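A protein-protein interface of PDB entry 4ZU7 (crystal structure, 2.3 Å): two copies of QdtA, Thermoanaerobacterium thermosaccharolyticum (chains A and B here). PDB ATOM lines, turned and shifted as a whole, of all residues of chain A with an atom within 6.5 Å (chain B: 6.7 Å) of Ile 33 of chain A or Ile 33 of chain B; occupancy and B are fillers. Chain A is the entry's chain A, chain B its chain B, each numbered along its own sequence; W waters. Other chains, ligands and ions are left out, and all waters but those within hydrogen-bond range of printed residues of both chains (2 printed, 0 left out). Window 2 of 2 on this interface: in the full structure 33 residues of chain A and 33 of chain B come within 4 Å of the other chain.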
ATOM      1  N   ILE A  23      24.859 -24.622  -7.910  1.00  0.00           N
ATOM      2  CA  ILE A  23      23.931 -23.614  -8.408  1.00  0.00           C
ATOM      3  C   ILE A  23      22.507 -23.859  -7.916  1.00  0.00           C
ATOM      4  O   ILE A  23      21.877 -24.848  -8.302  1.00  0.00           O
ATOM      5  CB  ILE A  23      24.012 -23.511  -9.913  1.00  0.00           C
ATOM      6  CG1 ILE A  23      25.454 -23.143 -10.309  1.00  0.00           C
ATOM      7  CG2 ILE A  23      23.087 -22.407 -10.428  1.00  0.00           C
ATOM      8  CD1 ILE A  23      25.844 -23.519 -11.713  1.00  0.00           C
ATOM      9  N   GLU A  24      22.020 -22.969  -7.025  1.00  0.00           N
ATOM     10  CA  GLU A  24      20.626 -23.016  -6.563  1.00  0.00           C
ATOM     11  C   GLU A  24      19.758 -22.087  -7.381  1.00  0.00           C
ATOM     12  O   GLU A  24      20.102 -20.920  -7.596  1.00  0.00           O
ATOM     13  CB  GLU A  24      20.523 -22.655  -5.076  1.00  0.00           C
ATOM     14  CG  GLU A  24      21.543 -23.361  -4.190  1.00  0.00           C
ATOM     15  CD  GLU A  24      21.210 -23.335  -2.712  1.00  0.00           C
ATOM     16  OE1 GLU A  24      20.695 -22.348  -2.174  1.00  0.00           O
ATOM     17  OE2 GLU A  24      21.484 -24.325  -2.067  1.00  0.00           O
ATOM     18  N   GLY A  25      18.629 -22.615  -7.850  1.00  0.00           N
ATOM     19  CA  GLY A  25      17.688 -21.849  -8.639  1.00  0.00           C
ATOM     20  C   GLY A  25      17.090 -20.666  -7.891  1.00  0.00           C
ATOM     21  O   GLY A  25      16.784 -20.747  -6.712  1.00  0.00           O
ATOM     22  N   LYS A  26      16.903 -19.567  -8.615  1.00  0.00           N
ATOM     23  CA  LYS A  26      16.507 -18.280  -8.043  1.00  0.00           C
ATOM     24  C   LYS A  26      17.505 -17.705  -7.065  1.00  0.00           C
ATOM     25  O   LYS A  26      17.375 -16.550  -6.708  1.00  0.00           O
ATOM     26  CB  LYS A  26      15.142 -18.346  -7.383  1.00  0.00           C
ATOM     27  CG  LYS A  26      14.076 -18.857  -8.324  1.00  0.00           C
ATOM     28  CD  LYS A  26      12.683 -18.706  -7.736  1.00  0.00           C
ATOM     29  CE  LYS A  26      12.525 -19.607  -6.532  1.00  0.00           C
ATOM     30  NZ  LYS A  26      11.092 -19.854  -6.243  1.00  0.00           N
ATOM     31  N   ILE A  29      21.429 -17.970  -9.732  1.00  0.00           N
ATOM     32  CA  ILE A  29      20.957 -17.465 -11.019  1.00  0.00           C
ATOM     33  C   ILE A  29      19.555 -16.892 -10.752  1.00  0.00           C
ATOM     34  O   ILE A  29      18.945 -17.226  -9.735  1.00  0.00           O
ATOM     35  CB  ILE A  29      20.861 -18.586 -12.043  1.00  0.00           C
ATOM     36  CG1 ILE A  29      19.934 -19.699 -11.568  1.00  0.00           C
ATOM     37  CG2 ILE A  29      22.226 -19.178 -12.258  1.00  0.00           C
ATOM     38  CD1 ILE A  29      19.547 -20.680 -12.659  1.00  0.00           C
ATOM     39  N   PHE A  31      16.487 -17.250 -12.095  1.00  0.00           N
ATOM     40  CA  PHE A  31      15.301 -18.057 -12.436  1.00  0.00           C
ATOM     41  C   PHE A  31      15.338 -19.473 -11.836  1.00  0.00           C
ATOM     42  O   PHE A  31      16.388 -19.948 -11.405  1.00  0.00           O
ATOM     43  CB  PHE A  31      15.109 -18.167 -13.988  1.00  0.00           C
ATOM     44  CG  PHE A  31      16.332 -18.707 -14.759  1.00  0.00           C
ATOM     45  CD1 PHE A  31      16.494 -20.063 -15.008  1.00  0.00           C
ATOM     46  CD2 PHE A  31      17.281 -17.841 -15.270  1.00  0.00           C
ATOM     47  CE1 PHE A  31      17.591 -20.553 -15.688  1.00  0.00           C
ATOM     48  CE2 PHE A  31      18.369 -18.322 -16.000  1.00  0.00           C
ATOM     49  CZ  PHE A  31      18.539 -19.677 -16.189  1.00  0.00           C
ATOM     50  N   ASP A  32      14.167 -20.119 -11.800  1.00  0.00           N
ATOM     51  CA  ASP A  32      14.029 -21.527 -11.429  1.00  0.00           C
ATOM     52  C   ASP A  32      14.449 -22.387 -12.598  1.00  0.00           C
ATOM     53  O   ASP A  32      14.196 -22.011 -13.726  1.00  0.00           O
ATOM     54  CB  ASP A  32      12.593 -21.918 -11.063  1.00  0.00           C
ATOM     55  CG  ASP A  32      12.306 -21.763  -9.601  1.00  0.00           C
ATOM     56  OD1 ASP A  32      13.188 -22.123  -8.791  1.00  0.00           O
ATOM     57  OD2 ASP A  32      11.201 -21.225  -9.256  1.00  0.00           O
ATOM     58  N   ILE A  33      15.043 -23.549 -12.286  1.00  0.00           N
ATOM     59  CA  ILE A  33      15.578 -24.462 -13.286  1.00  0.00           C
ATOM     60  C   ILE A  33      14.526 -25.475 -13.655  1.00  0.00           C
ATOM     61  O   ILE A  33      14.366 -26.480 -12.979  1.00  0.00           O
ATOM     62  CB  ILE A  33      16.825 -25.190 -12.729  1.00  0.00           C
ATOM     63  CG1 ILE A  33      17.911 -24.176 -12.440  1.00  0.00           C
ATOM     64  CG2 ILE A  33      17.375 -26.191 -13.728  1.00  0.00           C
ATOM     65  CD1 ILE A  33      19.077 -24.675 -11.625  1.00  0.00           C
ATOM     66  N   LYS A  34      13.806 -25.247 -14.743  1.00  0.00           N
ATOM     67  CA  LYS A  34      12.825 -26.237 -15.180  1.00  0.00           C
ATOM     68  C   LYS A  34      13.478 -27.363 -16.028  1.00  0.00           C
ATOM     69  O   LYS A  34      12.956 -28.451 -16.119  1.00  0.00           O
ATOM     70  CB  LYS A  34      11.676 -25.589 -15.933  1.00  0.00           C
ATOM     71  CG  LYS A  34      10.641 -24.853 -15.066  1.00  0.00           C
ATOM     72  CD  LYS A  34       9.198 -25.121 -15.520  1.00  0.00           C
ATOM     73  CE  LYS A  34       8.303 -23.882 -15.528  1.00  0.00           C
ATOM     74  NZ  LYS A  34       8.370 -23.053 -14.269  1.00  0.00           N
ATOM     75  N   ARG A  35      14.618 -27.079 -16.621  1.00  0.00           N
ATOM     76  CA  ARG A  35      15.224 -27.966 -17.588  1.00  0.00           C
ATOM     77  C   ARG A  35      16.704 -27.707 -17.627  1.00  0.00           C
ATOM     78  O   ARG A  35      17.118 -26.540 -17.483  1.00  0.00           O
ATOM     79  CB  ARG A  35      14.682 -27.656 -18.961  1.00  0.00           C
ATOM     80  CG  ARG A  35      15.483 -28.264 -20.080  1.00  0.00           C
ATOM     81  CD  ARG A  35      14.677 -28.162 -21.377  1.00  0.00           C
ATOM     82  NE  ARG A  35      14.375 -26.755 -21.723  1.00  0.00           N
ATOM     83  CZ  ARG A  35      14.859 -26.145 -22.789  1.00  0.00           C
ATOM     84  NH1 ARG A  35      14.534 -24.896 -23.008  1.00  0.00           N
ATOM     85  NH2 ARG A  35      15.671 -26.791 -23.645  1.00  0.00           N
ATOM     86  N   VAL A  36      17.490 -28.780 -17.758  1.00  0.00           N
ATOM     87  CA  VAL A  36      18.891 -28.635 -18.126  1.00  0.00           C
ATOM     88  C   VAL A  36      19.186 -29.390 -19.395  1.00  0.00           C
ATOM     89  O   VAL A  36      18.444 -30.294 -19.786  1.00  0.00           O
ATOM     90  CB  VAL A  36      19.904 -29.067 -17.046  1.00  0.00           C
ATOM     91  CG1 VAL A  36      19.558 -28.439 -15.718  1.00  0.00           C
ATOM     92  CG2 VAL A  36      19.957 -30.576 -16.915  1.00  0.00           C
ATOM     93  N   LEU A 111      21.503 -24.312 -18.267  1.00  0.00           N
ATOM     94  CA  LEU A 111      20.379 -24.250 -17.367  1.00  0.00           C
ATOM     95  C   LEU A 111      19.298 -23.350 -18.008  1.00  0.00           C
ATOM     96  O   LEU A 111      19.603 -22.265 -18.461  1.00  0.00           O
ATOM     97  CB  LEU A 111      20.816 -23.627 -16.034  1.00  0.00           C
ATOM     98  CG  LEU A 111      22.068 -24.092 -15.302  1.00  0.00           C
ATOM     99  CD1 LEU A 111      22.292 -23.314 -14.036  1.00  0.00           C
ATOM    100  CD2 LEU A 111      21.966 -25.535 -14.976  1.00  0.00           C
ATOM    101  N   ALA A 112      18.038 -23.757 -17.976  1.00  0.00           N
ATOM    102  CA  ALA A 112      16.967 -23.070 -18.693  1.00  0.00           C
ATOM    103  C   ALA A 112      15.670 -22.831 -17.853  1.00  0.00           C
ATOM    104  O   ALA A 112      15.246 -23.677 -17.023  1.00  0.00           O
ATOM    105  CB  ALA A 112      16.640 -23.864 -19.916  1.00  0.00           C
ATOM    106  N   SER A 113      15.027 -21.690 -18.063  1.00  0.00           N
ATOM    107  CA  SER A 113      13.833 -21.378 -17.249  1.00  0.00           C
ATOM    108  C   SER A 113      12.517 -22.012 -17.698  1.00  0.00           C
ATOM    109  O   SER A 113      11.578 -21.881 -17.017  1.00  0.00           O
ATOM    110  CB  SER A 113      13.628 -19.856 -17.096  1.00  0.00           C
ATOM    111  OG  SER A 113      13.650 -19.197 -18.320  1.00  0.00           O
ATOM    112  N   GLU A 114      12.445 -22.687 -18.838  1.00  0.00           N
ATOM    113  CA  GLU A 114      11.185 -23.314 -19.283  1.00  0.00           C
ATOM    114  C   GLU A 114      11.470 -24.673 -19.869  1.00  0.00           C
ATOM    115  O   GLU A 114      12.608 -24.985 -20.251  1.00  0.00           O
ATOM    116  CB  GLU A 114      10.482 -22.469 -20.367  1.00  0.00           C
ATOM    117  CG  GLU A 114      10.005 -21.090 -19.933  1.00  0.00           C
ATOM    118  CD  GLU A 114       9.054 -21.120 -18.724  1.00  0.00           C
ATOM    119  OE1 GLU A 114       8.290 -22.122 -18.528  1.00  0.00           O
ATOM    120  OE2 GLU A 114       9.127 -20.140 -17.960  1.00  0.00           O
ATOM    121  N   TYR A 115      10.431 -25.466 -20.015  1.00  0.00           N
ATOM    122  CA  TYR A 115      10.623 -26.753 -20.657  1.00  0.00           C
ATOM    123  C   TYR A 115      10.806 -26.421 -22.114  1.00  0.00           C
ATOM    124  O   TYR A 115      10.444 -25.323 -22.560  1.00  0.00           O
ATOM    125  CB  TYR A 115       9.435 -27.709 -20.469  1.00  0.00           C
ATOM    126  CG  TYR A 115       9.149 -28.211 -19.054  1.00  0.00           C
ATOM    127  CD1 TYR A 115       7.841 -28.437 -18.663  1.00  0.00           C
ATOM    128  CD2 TYR A 115      10.165 -28.506 -18.137  1.00  0.00           C
ATOM    129  CE1 TYR A 115       7.537 -28.905 -17.402  1.00  0.00           C
ATOM    130  CE2 TYR A 115       9.880 -28.985 -16.864  1.00  0.00           C
ATOM    131  CZ  TYR A 115       8.562 -29.171 -16.494  1.00  0.00           C
ATOM    132  OH  TYR A 115       8.175 -29.618 -15.243  1.00  0.00           O
ATOM    133  N   ILE B  23      17.215 -32.761 -20.050  1.00  0.00           N
ATOM    134  CA  ILE B  23      16.555 -33.313 -18.847  1.00  0.00           C
ATOM    135  C   ILE B  23      15.557 -32.254 -18.335  1.00  0.00           C
ATOM    136  O   ILE B  23      15.940 -31.113 -17.997  1.00  0.00           O
ATOM    137  CB  ILE B  23      17.586 -33.638 -17.745  1.00  0.00           C
ATOM    138  CG1 ILE B  23      18.697 -34.533 -18.286  1.00  0.00           C
ATOM    139  CG2 ILE B  23      16.942 -34.342 -16.579  1.00  0.00           C
ATOM    140  CD1 ILE B  23      19.795 -34.861 -17.311  1.00  0.00           C
ATOM    141  N   GLU B  24      14.271 -32.608 -18.317  1.00  0.00           N
ATOM    142  CA  GLU B  24      13.224 -31.711 -17.800  1.00  0.00           C
ATOM    143  C   GLU B  24      12.790 -32.226 -16.456  1.00  0.00           C
ATOM    144  O   GLU B  24      12.505 -33.418 -16.296  1.00  0.00           O
ATOM    145  CB  GLU B  24      12.053 -31.635 -18.773  1.00  0.00           C
ATOM    146  CG  GLU B  24      12.476 -31.141 -20.156  1.00  0.00           C
ATOM    147  CD  GLU B  24      11.353 -31.079 -21.147  1.00  0.00           C
ATOM    148  OE1 GLU B  24      10.543 -32.023 -21.204  1.00  0.00           O
ATOM    149  OE2 GLU B  24      11.298 -30.081 -21.894  1.00  0.00           O
ATOM    150  N   GLY B  25      12.825 -31.354 -15.464  1.00  0.00           N
ATOM    151  CA  GLY B  25      12.366 -31.714 -14.124  1.00  0.00           C
ATOM    152  C   GLY B  25      10.969 -32.323 -14.113  1.00  0.00           C
ATOM    153  O   GLY B  25      10.119 -31.958 -14.940  1.00  0.00           O
ATOM    154  N   LYS B  26      10.757 -33.283 -13.199  1.00  0.00           N
ATOM    155  CA  LYS B  26       9.499 -34.042 -13.083  1.00  0.00           C
ATOM    156  C   LYS B  26       9.214 -34.937 -14.270  1.00  0.00           C
ATOM    157  O   LYS B  26       8.440 -35.876 -14.154  1.00  0.00           O
ATOM    158  CB  LYS B  26       8.281 -33.140 -12.843  1.00  0.00           C
ATOM    159  CG  LYS B  26       8.255 -32.477 -11.485  1.00  0.00           C
ATOM    160  CD  LYS B  26       6.911 -31.785 -11.192  1.00  0.00           C
ATOM    161  CE  LYS B  26       6.549 -30.762 -12.269  1.00  0.00           C
ATOM    162  NZ  LYS B  26       5.781 -29.599 -11.733  1.00  0.00           N
ATOM    163  N   ILE B  29      13.546 -36.910 -15.017  1.00  0.00           N
ATOM    164  CA  ILE B  29      13.798 -37.392 -13.684  1.00  0.00           C
ATOM    165  C   ILE B  29      12.509 -37.210 -12.919  1.00  0.00           C
ATOM    166  O   ILE B  29      11.635 -36.497 -13.367  1.00  0.00           O
ATOM    167  CB  ILE B  29      14.935 -36.655 -12.989  1.00  0.00           C
ATOM    168  CG1 ILE B  29      14.724 -35.138 -12.989  1.00  0.00           C
ATOM    169  CG2 ILE B  29      16.234 -36.998 -13.693  1.00  0.00           C
ATOM    170  CD1 ILE B  29      15.819 -34.372 -12.240  1.00  0.00           C
ATOM    171  N   PHE B  31      11.807 -35.704 -10.169  1.00  0.00           N
ATOM    172  CA  PHE B  31      11.623 -34.597  -9.246  1.00  0.00           C
ATOM    173  C   PHE B  31      11.925 -33.322  -9.952  1.00  0.00           C
ATOM    174  O   PHE B  31      12.353 -33.356 -11.097  1.00  0.00           O
ATOM    175  CB  PHE B  31      12.461 -34.795  -7.986  1.00  0.00           C
ATOM    176  CG  PHE B  31      13.928 -34.938  -8.242  1.00  0.00           C
ATOM    177  CD1 PHE B  31      14.751 -33.807  -8.307  1.00  0.00           C
ATOM    178  CD2 PHE B  31      14.494 -36.184  -8.371  1.00  0.00           C
ATOM    179  CE1 PHE B  31      16.119 -33.927  -8.518  1.00  0.00           C
ATOM    180  CE2 PHE B  31      15.859 -36.306  -8.562  1.00  0.00           C
ATOM    181  CZ  PHE B  31      16.677 -35.178  -8.658  1.00  0.00           C
ATOM    182  N   ASP B  32      11.579 -32.224  -9.293  1.00  0.00           N
ATOM    183  CA  ASP B  32      11.847 -30.861  -9.736  1.00  0.00           C
ATOM    184  C   ASP B  32      13.242 -30.509  -9.298  1.00  0.00           C
ATOM    185  O   ASP B  32      13.645 -30.869  -8.188  1.00  0.00           O
ATOM    186  CB  ASP B  32      10.876 -29.856  -9.075  1.00  0.00           C
ATOM    187  CG  ASP B  32       9.654 -29.564  -9.930  1.00  0.00           C
ATOM    188  OD1 ASP B  32       9.797 -29.372 -11.169  1.00  0.00           O
ATOM    189  OD2 ASP B  32       8.545 -29.513  -9.344  1.00  0.00           O
ATOM    190  N   ILE B  33      13.938 -29.756 -10.137  1.00  0.00           N
ATOM    191  CA  ILE B  33      15.334 -29.462  -9.933  1.00  0.00           C
ATOM    192  C   ILE B  33      15.492 -28.135  -9.198  1.00  0.00           C
ATOM    193  O   ILE B  33      15.305 -27.094  -9.797  1.00  0.00           O
ATOM    194  CB  ILE B  33      16.079 -29.358 -11.292  1.00  0.00           C
ATOM    195  CG1 ILE B  33      15.945 -30.638 -12.104  1.00  0.00           C
ATOM    196  CG2 ILE B  33      17.554 -29.124 -11.080  1.00  0.00           C
ATOM    197  CD1 ILE B  33      16.526 -30.524 -13.515  1.00  0.00           C
ATOM    198  N   LYS B  34      15.902 -28.156  -7.931  1.00  0.00           N
ATOM    199  CA  LYS B  34      16.099 -26.923  -7.206  1.00  0.00           C
ATOM    200  C   LYS B  34      17.535 -26.486  -7.165  1.00  0.00           C
ATOM    201  O   LYS B  34      17.813 -25.322  -6.919  1.00  0.00           O
ATOM    202  CB  LYS B  34      15.534 -27.055  -5.786  1.00  0.00           C
ATOM    203  CG  LYS B  34      14.095 -26.537  -5.698  1.00  0.00           C
ATOM    204  CD  LYS B  34      13.257 -27.207  -4.627  1.00  0.00           C
ATOM    205  CE  LYS B  34      13.081 -26.331  -3.381  1.00  0.00           C
ATOM    206  NZ  LYS B  34      11.646 -26.271  -2.936  1.00  0.00           N
ATOM    207  N   ARG B  35      18.447 -27.422  -7.362  1.00  0.00           N
ATOM    208  CA  ARG B  35      19.872 -27.138  -7.269  1.00  0.00           C
ATOM    209  C   ARG B  35      20.622 -28.116  -8.166  1.00  0.00           C
ATOM    210  O   ARG B  35      20.235 -29.262  -8.213  1.00  0.00           O
ATOM    211  CB  ARG B  35      20.356 -27.350  -5.858  1.00  0.00           C
ATOM    212  CG  ARG B  35      21.883 -27.396  -5.696  1.00  0.00           C
ATOM    213  CD  ARG B  35      22.226 -27.495  -4.218  1.00  0.00           C
ATOM    214  NE  ARG B  35      21.463 -28.590  -3.609  1.00  0.00           N
ATOM    215  CZ  ARG B  35      21.988 -29.560  -2.882  1.00  0.00           C
ATOM    216  NH1 ARG B  35      21.199 -30.515  -2.398  1.00  0.00           N
ATOM    217  NH2 ARG B  35      23.299 -29.589  -2.609  1.00  0.00           N
ATOM    218  N   VAL B  36      21.652 -27.652  -8.890  1.00  0.00           N
ATOM    219  CA  VAL B  36      22.603 -28.559  -9.522  1.00  0.00           C
ATOM    220  C   VAL B  36      23.925 -28.248  -8.928  1.00  0.00           C
ATOM    221  O   VAL B  36      24.132 -27.125  -8.459  1.00  0.00           O
ATOM    222  CB  VAL B  36      22.771 -28.400 -11.046  1.00  0.00           C
ATOM    223  CG1 VAL B  36      21.439 -28.401 -11.771  1.00  0.00           C
ATOM    224  CG2 VAL B  36      23.585 -27.159 -11.393  1.00  0.00           C
ATOM    225  N   VAL B 110      25.470 -33.296 -10.616  1.00  0.00           N
ATOM    226  CA  VAL B 110      24.437 -33.801  -9.723  1.00  0.00           C
ATOM    227  C   VAL B 110      23.198 -32.929  -9.803  1.00  0.00           C
ATOM    228  O   VAL B 110      23.293 -31.706  -9.718  1.00  0.00           O
ATOM    229  CB  VAL B 110      24.917 -33.810  -8.283  1.00  0.00           C
ATOM    230  CG1 VAL B 110      23.912 -34.465  -7.372  1.00  0.00           C
ATOM    231  CG2 VAL B 110      26.220 -34.566  -8.187  1.00  0.00           C
ATOM    232  N   LEU B 111      22.050 -33.551 -10.036  1.00  0.00           N
ATOM    233  CA  LEU B 111      20.802 -32.816 -10.008  1.00  0.00           C
ATOM    234  C   LEU B 111      20.194 -33.108  -8.648  1.00  0.00           C
ATOM    235  O   LEU B 111      20.291 -34.244  -8.199  1.00  0.00           O
ATOM    236  CB  LEU B 111      19.869 -33.248 -11.137  1.00  0.00           C
ATOM    237  CG  LEU B 111      20.485 -33.249 -12.545  1.00  0.00           C
ATOM    238  CD1 LEU B 111      19.464 -33.603 -13.631  1.00  0.00           C
ATOM    239  CD2 LEU B 111      21.195 -31.956 -12.851  1.00  0.00           C
ATOM    240  N   ALA B 112      19.587 -32.101  -8.006  1.00  0.00           N
ATOM    241  CA  ALA B 112      19.139 -32.214  -6.600  1.00  0.00           C
ATOM    242  C   ALA B 112      17.724 -31.632  -6.336  1.00  0.00           C
ATOM    243  O   ALA B 112      17.430 -30.478  -6.661  1.00  0.00           O
ATOM    244  CB  ALA B 112      20.141 -31.527  -5.690  1.00  0.00           C
ATOM    245  N   SER B 113      16.892 -32.417  -5.668  1.00  0.00           N
ATOM    246  CA  SER B 113      15.525 -32.010  -5.335  1.00  0.00           C
ATOM    247  C   SER B 113      15.362 -30.837  -4.366  1.00  0.00           C
ATOM    248  O   SER B 113      14.257 -30.298  -4.247  1.00  0.00           O
ATOM    249  CB  SER B 113      14.731 -33.214  -4.822  1.00  0.00           C
ATOM    250  OG  SER B 113      15.210 -33.743  -3.592  1.00  0.00           O
ATOM    251  N   GLU B 114      16.430 -30.433  -3.679  1.00  0.00           N
ATOM    252  CA  GLU B 114      16.309 -29.413  -2.624  1.00  0.00           C
ATOM    253  C   GLU B 114      17.565 -28.547  -2.589  1.00  0.00           C
ATOM    254  O   GLU B 114      18.639 -28.967  -3.011  1.00  0.00           O
ATOM    255  CB  GLU B 114      16.178 -30.066  -1.237  1.00  0.00           C
ATOM    256  CG  GLU B 114      14.905 -30.886  -0.962  1.00  0.00           C
ATOM    257  CD  GLU B 114      13.578 -30.079  -1.036  1.00  0.00           C
ATOM    258  OE1 GLU B 114      13.634 -28.803  -0.976  1.00  0.00           O
ATOM    259  OE2 GLU B 114      12.485 -30.738  -1.168  1.00  0.00           O
HETATM  260  O   HOH W   1      12.869 -28.852 -12.372  1.00  0.00           O
HETATM  261  O   HOH W   2      15.655 -24.296  -9.665  1.00  0.00           O
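Ile 23 of chain A touches Arg 35 of chain B (O to CA, 3.2 Å). CA of Glu 24 of chain A touches O of Lys 34 of chain B (3.7 Å). Arg 35 of chain B touches Glu 24 of chain A (CD to OE2, 3.9 Å). Lys 34 of chain A touches Glu 24 of chain B. Ile 23 of chain B touches Arg 35 of chain A (O to CA, 3.3 Å). Arg 35 of chain A touches Glu 24 of chain B (CD to CG, 3.9 Å). Glu 24 of chain B touches Tyr 115 of chain A. Lys 26 of chain B touches Tyr 115 of chain A (CE to OH, 3.6 Å).
Ile 23 of chain A touches Arg 35 of chain B, and with the chains exchanged Arg 35 of chain A touches Ile 23 of chain B. Glu 24 of chain A touches Lys 34 of chain B, and with the chains exchanged Lys 34 of chain A touches Glu 24 of chain B. Gly 25 of chain A touches Lys 34 of chain B, and with the chains exchanged Lys 34 of chain A touches Gly 25 of chain B. Ile 33 of chain B touches its own counterpart, Ile 33 of chain A. Of the 14 pairs that touch across the chains among the printed residues, 11 have their exchanged pair printed and touching as well.
N of Ile 23 of chain A lies within hydrogen-bond range of O of Val 36 of chain B, 2.7 Å away. N of Gly 25 of chain A sits at hydrogen-bond distance from O of Lys 34 of chain B (3.0 Å). O of Lys 34 of chain A sits at hydrogen-bond distance from N of Gly 25 of chain B, 3.0 Å away. N of Ile 23 of chain B lies within hydrogen-bond range of O of Val 36 of chain A, at 2.8 Å. OH of Tyr 115 of chain A lies within hydrogen-bond range of O of Gly 25 of chain B (3.1 Å). O of Ile 33 of chain B sits close to O of Ile 33 of chain A.
Water W1 lies within hydrogen-bond range of the backbone NH (N) of Ile 33 of chain B (2.6 Å), the backbone carbonyl oxygen (O) of Ile 33 of chain A (2.9 Å) and the side-chain carboxylate (OD1) of Asp 32 of chain B (3.3 Å). Water W2 lies within hydrogen-bond range of the backbone NH of Ile 33 of chain A (2.8 Å), the backbone carbonyl oxygen of Ile 33 of chain B (2.8 Å) and the side-chain carboxylate of Asp 32 of chain A (3.4 Å).
Printed residues of chain B that touch a printed residue of chain A: Ile 23, Glu 24, Gly 25, Lys 26, Ile 33, Lys 34, Arg 35 and Val 36. Along chain A the printed residues that touch a printed residue of chain B span positions 23 to 115. Among the printed residues, no Asp or Glu carboxylate lies within 4 Å of a Lys or Arg side-chain nitrogen of the other chain.
N of Lys 34 of chain A is in hydrogen-bond range of O of Ala 112 of chain A. The backbone NH of Ala 112 of chain A is in hydrogen-bond range of the backbone carbonyl oxygen of Arg 35 of chain A, at 3.0 Å. NE of Arg 35 of chain A lies within hydrogen-bond range of O of Glu 114 of chain A, 2.9 Å away. The backbone NH of Lys 26 of chain B lies within hydrogen-bond range of the backbone carbonyl oxygen of Phe 31 of chain B (2.6 Å). OD2 of Asp 32 of chain B is in salt-bridge range of NZ of Lys 26 of chain B (3.7 Å). The backbone NH of Lys 34 of chain B is in hydrogen-bond range of the backbone carbonyl oxygen of Ala 112 of chain B (3.1 Å).
Of chain B, only Ile 33 comes within 4 Å of Ile 33 of chain A. Ile 33 of chain B touches just one residue of chain A: Ile 33. Printed residues of chain A within 4 Å of Val 36 of chain B: Ile 23 (2.7 Å). Of the printed residues of chain A, Arg 35 of chain B touches Ile 23 (3.2 Å) and Glu 24 (3.9 Å). Of the printed residues of chain A, Ile 23 of chain B touches Arg 35 and Val 36. Of the printed residues of chain B, Tyr 115 of chain A touches Glu 24, Gly 25 and Lys 26. Ala 112 of chain A touches none of the printed residues of chain B. The nearest residue of chain B that does not touch Ile 33 of chain A is Val 36 of chain B (4.4 Å).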
